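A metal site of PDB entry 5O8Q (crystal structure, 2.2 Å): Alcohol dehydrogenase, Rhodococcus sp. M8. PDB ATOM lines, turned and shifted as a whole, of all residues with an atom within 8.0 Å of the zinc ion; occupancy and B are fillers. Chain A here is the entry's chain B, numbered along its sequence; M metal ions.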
ATOM      1  N   TRP A  90       0.165 -28.006  11.254  1.00  0.00           N
ATOM      2  CA  TRP A  90      -1.190 -28.248  10.747  1.00  0.00           C
ATOM      3  C   TRP A  90      -1.868 -26.970  10.258  1.00  0.00           C
ATOM      4  O   TRP A  90      -1.928 -25.974  10.985  1.00  0.00           O
ATOM      5  CB  TRP A  90      -2.082 -28.923  11.812  1.00  0.00           C
ATOM      6  CG  TRP A  90      -1.659 -30.298  12.260  1.00  0.00           C
ATOM      7  CD1 TRP A  90      -0.684 -31.065  11.718  1.00  0.00           C
ATOM      8  CD2 TRP A  90      -2.238 -31.072  13.324  1.00  0.00           C
ATOM      9  NE1 TRP A  90      -0.582 -32.266  12.395  1.00  0.00           N
ATOM     10  CE2 TRP A  90      -1.536 -32.294  13.374  1.00  0.00           C
ATOM     11  CE3 TRP A  90      -3.278 -30.848  14.229  1.00  0.00           C
ATOM     12  CZ2 TRP A  90      -1.823 -33.292  14.314  1.00  0.00           C
ATOM     13  CZ3 TRP A  90      -3.582 -31.846  15.173  1.00  0.00           C
ATOM     14  CH2 TRP A  90      -2.844 -33.058  15.222  1.00  0.00           C
ATOM     15  N   GLY A  91      -2.369 -27.013   9.017  1.00  0.00           N
ATOM     16  CA  GLY A  91      -3.091 -25.893   8.404  1.00  0.00           C
ATOM     17  C   GLY A  91      -4.563 -26.250   8.233  1.00  0.00           C
ATOM     18  O   GLY A  91      -4.995 -27.329   8.636  1.00  0.00           O
ATOM     19  N   CYS A  92      -5.332 -25.332   7.631  1.00  0.00           N
ATOM     20  CA  CYS A  92      -6.754 -25.553   7.404  1.00  0.00           C
ATOM     21  C   CYS A  92      -7.036 -26.600   6.303  1.00  0.00           C
ATOM     22  O   CYS A  92      -8.106 -27.195   6.272  1.00  0.00           O
ATOM     23  CB  CYS A  92      -7.451 -24.231   7.050  1.00  0.00           C
ATOM     24  SG  CYS A  92      -7.129 -23.567   5.395  1.00  0.00           S
ATOM     25  N   GLY A  93      -6.082 -26.797   5.393  1.00  0.00           N
ATOM     26  CA  GLY A  93      -6.234 -27.754   4.300  1.00  0.00           C
ATOM     27  C   GLY A  93      -6.995 -27.261   3.079  1.00  0.00           C
ATOM     28  O   GLY A  93      -7.052 -27.987   2.072  1.00  0.00           O
ATOM     29  N   ALA A  94      -7.537 -26.032   3.140  1.00  0.00           N
ATOM     30  CA  ALA A  94      -8.468 -25.518   2.116  1.00  0.00           C
ATOM     31  C   ALA A  94      -8.043 -24.229   1.404  1.00  0.00           C
ATOM     32  O   ALA A  94      -8.547 -23.964   0.322  1.00  0.00           O
ATOM     33  CB  ALA A  94      -9.850 -25.306   2.745  1.00  0.00           C
ATOM     34  N   CYS A  95      -7.152 -23.419   1.990  1.00  0.00           N
ATOM     35  CA  CYS A  95      -6.719 -22.145   1.385  1.00  0.00           C
ATOM     36  C   CYS A  95      -5.704 -22.356   0.257  1.00  0.00           C
ATOM     37  O   CYS A  95      -5.213 -23.462   0.063  1.00  0.00           O
ATOM     38  CB  CYS A  95      -6.115 -21.204   2.458  1.00  0.00           C
ATOM     39  SG  CYS A  95      -4.517 -21.707   3.135  1.00  0.00           S
ATOM     40  N   HIS A  96      -5.385 -21.287  -0.460  1.00  0.00           N
ATOM     41  CA  HIS A  96      -4.452 -21.348  -1.585  1.00  0.00           C
ATOM     42  C   HIS A  96      -3.100 -21.935  -1.160  1.00  0.00           C
ATOM     43  O   HIS A  96      -2.566 -22.812  -1.862  1.00  0.00           O
ATOM     44  CB  HIS A  96      -4.276 -19.955  -2.187  1.00  0.00           C
ATOM     45  CG  HIS A  96      -3.534 -19.927  -3.486  1.00  0.00           C
ATOM     46  ND1 HIS A  96      -2.204 -19.556  -3.569  1.00  0.00           N
ATOM     47  CD2 HIS A  96      -3.930 -20.201  -4.752  1.00  0.00           C
ATOM     48  CE1 HIS A  96      -1.820 -19.594  -4.834  1.00  0.00           C
ATOM     49  NE2 HIS A  96      -2.842 -19.995  -5.570  1.00  0.00           N
ATOM     50  N   ALA A  97      -2.576 -21.510  -0.015  1.00  0.00           N
ATOM     51  CA  ALA A  97      -1.323 -22.069   0.498  1.00  0.00           C
ATOM     52  C   ALA A  97      -1.453 -23.569   0.817  1.00  0.00           C
ATOM     53  O   ALA A  97      -0.627 -24.358   0.360  1.00  0.00           O
ATOM     54  CB  ALA A  97      -0.841 -21.296   1.733  1.00  0.00           C
ATOM     55  N   CYS A  98      -2.503 -23.944   1.568  1.00  0.00           N
ATOM     56  CA  CYS A  98      -2.705 -25.349   1.942  1.00  0.00           C
ATOM     57  C   CYS A  98      -2.958 -26.258   0.732  1.00  0.00           C
ATOM     58  O   CYS A  98      -2.556 -27.430   0.724  1.00  0.00           O
ATOM     59  CB  CYS A  98      -3.860 -25.487   2.959  1.00  0.00           C
ATOM     60  SG  CYS A  98      -3.457 -24.917   4.635  1.00  0.00           S
ATOM     61  N   ALA A  99      -3.613 -25.728  -0.296  1.00  0.00           N
ATOM     62  CA  ALA A  99      -3.861 -26.490  -1.516  1.00  0.00           C
ATOM     63  C   ALA A  99      -2.571 -26.887  -2.244  1.00  0.00           C
ATOM     64  O   ALA A  99      -2.568 -27.876  -2.983  1.00  0.00           O
ATOM     65  CB  ALA A  99      -4.784 -25.717  -2.461  1.00  0.00           C
ATOM     66  N   ARG A 102       1.453 -26.184   1.380  1.00  0.00           N
ATOM     67  CA  ARG A 102       2.254 -25.239   2.147  1.00  0.00           C
ATOM     68  C   ARG A 102       1.496 -24.842   3.400  1.00  0.00           C
ATOM     69  O   ARG A 102       1.235 -23.671   3.636  1.00  0.00           O
ATOM     70  CB  ARG A 102       2.606 -23.997   1.312  1.00  0.00           C
ATOM     71  CG  ARG A 102       3.258 -24.316  -0.013  1.00  0.00           C
ATOM     72  CD  ARG A 102       3.418 -23.081  -0.905  1.00  0.00           C
ATOM     73  NE  ARG A 102       4.460 -22.163  -0.440  1.00  0.00           N
ATOM     74  CZ  ARG A 102       5.782 -22.354  -0.589  1.00  0.00           C
ATOM     75  NH1 ARG A 102       6.263 -23.451  -1.177  1.00  0.00           N
ATOM     76  NH2 ARG A 102       6.625 -21.461  -0.100  1.00  0.00           N
ATOM     77  N   GLU A 103       1.164 -25.835   4.234  1.00  0.00           N
ATOM     78  CA  GLU A 103       0.358 -25.604   5.430  1.00  0.00           C
ATOM     79  C   GLU A 103       1.135 -24.820   6.503  1.00  0.00           C
ATOM     80  O   GLU A 103       0.537 -24.191   7.379  1.00  0.00           O
ATOM     81  CB  GLU A 103      -0.163 -26.925   6.007  1.00  0.00           C
ATOM     82  CG  GLU A 103      -1.000 -27.724   5.017  1.00  0.00           C
ATOM     83  CD  GLU A 103      -1.953 -28.729   5.650  1.00  0.00           C
ATOM     84  OE1 GLU A 103      -2.090 -28.778   6.899  1.00  0.00           O
ATOM     85  OE2 GLU A 103      -2.597 -29.467   4.877  1.00  0.00           O
ATOM     86  N   ASN A 104       2.459 -24.848   6.417  1.00  0.00           N
ATOM     87  CA  ASN A 104       3.325 -23.975   7.218  1.00  0.00           C
ATOM     88  C   ASN A 104       3.034 -22.479   7.025  1.00  0.00           C
ATOM     89  O   ASN A 104       3.247 -21.686   7.945  1.00  0.00           O
ATOM     90  CB  ASN A 104       4.817 -24.272   6.998  1.00  0.00           C
ATOM     91  CG  ASN A 104       5.246 -24.199   5.539  1.00  0.00           C
ATOM     92  OD1 ASN A 104       4.496 -24.584   4.642  1.00  0.00           O
ATOM     93  ND2 ASN A 104       6.476 -23.732   5.301  1.00  0.00           N
ATOM     94  N   TYR A 105       2.524 -22.101   5.840  1.00  0.00           N
ATOM     95  CA  TYR A 105       2.129 -20.730   5.547  1.00  0.00           C
ATOM     96  C   TYR A 105       0.611 -20.549   5.406  1.00  0.00           C
ATOM     97  O   TYR A 105       0.151 -19.642   4.710  1.00  0.00           O
ATOM     98  CB  TYR A 105       2.871 -20.261   4.291  1.00  0.00           C
ATOM     99  CG  TYR A 105       4.391 -20.305   4.414  1.00  0.00           C
ATOM    100  CD1 TYR A 105       5.046 -19.766   5.527  1.00  0.00           C
ATOM    101  CD2 TYR A 105       5.187 -20.862   3.411  1.00  0.00           C
ATOM    102  CE1 TYR A 105       6.420 -19.764   5.627  1.00  0.00           C
ATOM    103  CE2 TYR A 105       6.577 -20.884   3.524  1.00  0.00           C
ATOM    104  CZ  TYR A 105       7.190 -20.326   4.638  1.00  0.00           C
ATOM    105  OH  TYR A 105       8.562 -20.358   4.770  1.00  0.00           O
ATOM    106  N   CYS A 106      -0.166 -21.384   6.097  1.00  0.00           N
ATOM    107  CA  CYS A 106      -1.620 -21.286   6.071  1.00  0.00           C
ATOM    108  C   CYS A 106      -2.050 -19.928   6.620  1.00  0.00           C
ATOM    109  O   CYS A 106      -1.613 -19.526   7.696  1.00  0.00           O
ATOM    110  CB  CYS A 106      -2.271 -22.375   6.928  1.00  0.00           C
ATOM    111  SG  CYS A 106      -4.079 -22.245   7.007  1.00  0.00           S
ATOM    112  N   THR A 107      -2.925 -19.247   5.875  1.00  0.00           N
ATOM    113  CA  THR A 107      -3.403 -17.908   6.225  1.00  0.00           C
ATOM    114  C   THR A 107      -4.645 -17.907   7.146  1.00  0.00           C
ATOM    115  O   THR A 107      -5.094 -16.840   7.522  1.00  0.00           O
ATOM    116  CB  THR A 107      -3.730 -17.106   4.935  1.00  0.00           C
ATOM    117  OG1 THR A 107      -4.493 -17.921   4.031  1.00  0.00           O
ATOM    118  CG2 THR A 107      -2.432 -16.679   4.225  1.00  0.00           C
ATOM    119  N   ARG A 108      -5.185 -19.082   7.494  1.00  0.00           N
ATOM    120  CA  ARG A 108      -6.473 -19.228   8.189  1.00  0.00           C
ATOM    121  C   ARG A 108      -6.469 -20.048   9.489  1.00  0.00           C
ATOM    122  O   ARG A 108      -7.497 -20.090  10.202  1.00  0.00           O
ATOM    123  CB  ARG A 108      -7.485 -19.905   7.252  1.00  0.00           C
ATOM    124  CG  ARG A 108      -7.892 -19.078   6.036  1.00  0.00           C
ATOM    125  CD  ARG A 108      -8.820 -19.919   5.147  1.00  0.00           C
ATOM    126  NE  ARG A 108     -10.098 -20.236   5.797  1.00  0.00           N
ATOM    127  CZ  ARG A 108     -11.005 -21.118   5.337  1.00  0.00           C
ATOM    128  NH1 ARG A 108     -12.137 -21.295   6.009  1.00  0.00           N
ATOM    129  NH2 ARG A 108     -10.769 -21.830   4.223  1.00  0.00           N
ATOM    130  N   ALA A 109      -5.367 -20.725   9.806  1.00  0.00           N
ATOM    131  CA  ALA A 109      -5.328 -21.677  10.928  1.00  0.00           C
ATOM    132  C   ALA A 109      -5.579 -21.009  12.293  1.00  0.00           C
ATOM    133  O   ALA A 109      -6.269 -21.579  13.145  1.00  0.00           O
ATOM    134  CB  ALA A 109      -4.012 -22.437  10.938  1.00  0.00           C
ATOM    135  N   LEU A 112      -9.338 -20.253  12.802  1.00  0.00           N
ATOM    136  CA  LEU A 112     -10.140 -21.499  12.945  1.00  0.00           C
ATOM    137  C   LEU A 112      -9.826 -22.317  14.213  1.00  0.00           C
ATOM    138  O   LEU A 112     -10.482 -23.331  14.471  1.00  0.00           O
ATOM    139  CB  LEU A 112      -9.967 -22.393  11.686  1.00  0.00           C
ATOM    140  CG  LEU A 112     -10.741 -21.967  10.424  1.00  0.00           C
ATOM    141  CD1 LEU A 112     -10.308 -22.818   9.246  1.00  0.00           C
ATOM    142  CD2 LEU A 112     -12.252 -22.071  10.615  1.00  0.00           C
ATOM    143  N   ILE A 114      -6.986 -24.052  14.829  1.00  0.00           N
ATOM    144  CA  ILE A 114      -6.181 -25.236  14.517  1.00  0.00           C
ATOM    145  C   ILE A 114      -4.794 -24.967  15.049  1.00  0.00           C
ATOM    146  O   ILE A 114      -4.125 -24.018  14.617  1.00  0.00           O
ATOM    147  CB  ILE A 114      -6.173 -25.560  12.992  1.00  0.00           C
ATOM    148  CG1 ILE A 114      -7.570 -26.045  12.555  1.00  0.00           C
ATOM    149  CG2 ILE A 114      -5.146 -26.637  12.673  1.00  0.00           C
ATOM    150  CD1 ILE A 114      -7.779 -26.116  11.063  1.00  0.00           C
ATOM    151  N   ARG A 135      -3.936 -36.659   5.875  1.00  0.00           N
ATOM    152  CA  ARG A 135      -2.962 -35.875   5.138  1.00  0.00           C
ATOM    153  C   ARG A 135      -1.759 -35.395   5.993  1.00  0.00           C
ATOM    154  O   ARG A 135      -0.764 -34.922   5.436  1.00  0.00           O
ATOM    155  CB  ARG A 135      -3.626 -34.674   4.434  1.00  0.00           C
ATOM    156  CG  ARG A 135      -3.996 -33.515   5.331  1.00  0.00           C
ATOM    157  CD  ARG A 135      -4.644 -32.380   4.564  1.00  0.00           C
ATOM    158  NE  ARG A 135      -4.713 -31.162   5.376  1.00  0.00           N
ATOM    159  CZ  ARG A 135      -5.637 -30.913   6.303  1.00  0.00           C
ATOM    160  NH1 ARG A 135      -6.624 -31.764   6.580  1.00  0.00           N
ATOM    161  NH2 ARG A 135      -5.566 -29.780   7.004  1.00  0.00           N
HETATM  162 ZN    ZN M   1      -4.844 -23.116   4.936  1.00  0.00          ZN
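SG of Cys 98 sits close to N of Gly 93, 3.3 Å away.
The side-chain sulfur (SG) of Cys 95 lies close to the backbone NH (N) of Ala 97 (3.7 Å).
The side-chain sulfur (SG) of Cys 92 lies close to the backbone NH (N) of Ala 94 (3.4 Å).
SG of Cys 106 sits close to N of Arg 108, at 3.4 Å.
SG of Cys 106 sits close to N of Ala 109, 3.4 Å away.
Gly 93 touches the zinc ion (N to ZN, 3.9 Å).
Along chain A the residues within 4 Å of the zinc ion span positions 92 to 106.
The nearest printed residue that does not touch the zinc ion is Ala 94 (4.4 Å).
SG of Cys 98 binds the zinc ion (2.3 Å).
The zinc ion is bound by SG of Cys 95.
SG of Cys 92 is bound to the zinc ion (2.4 Å).
The zinc ion is bound by the side-chain sulfur (SG) of Cys 106, at 2.4 Å.
The zinc ion has four donor atoms within binding distance.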
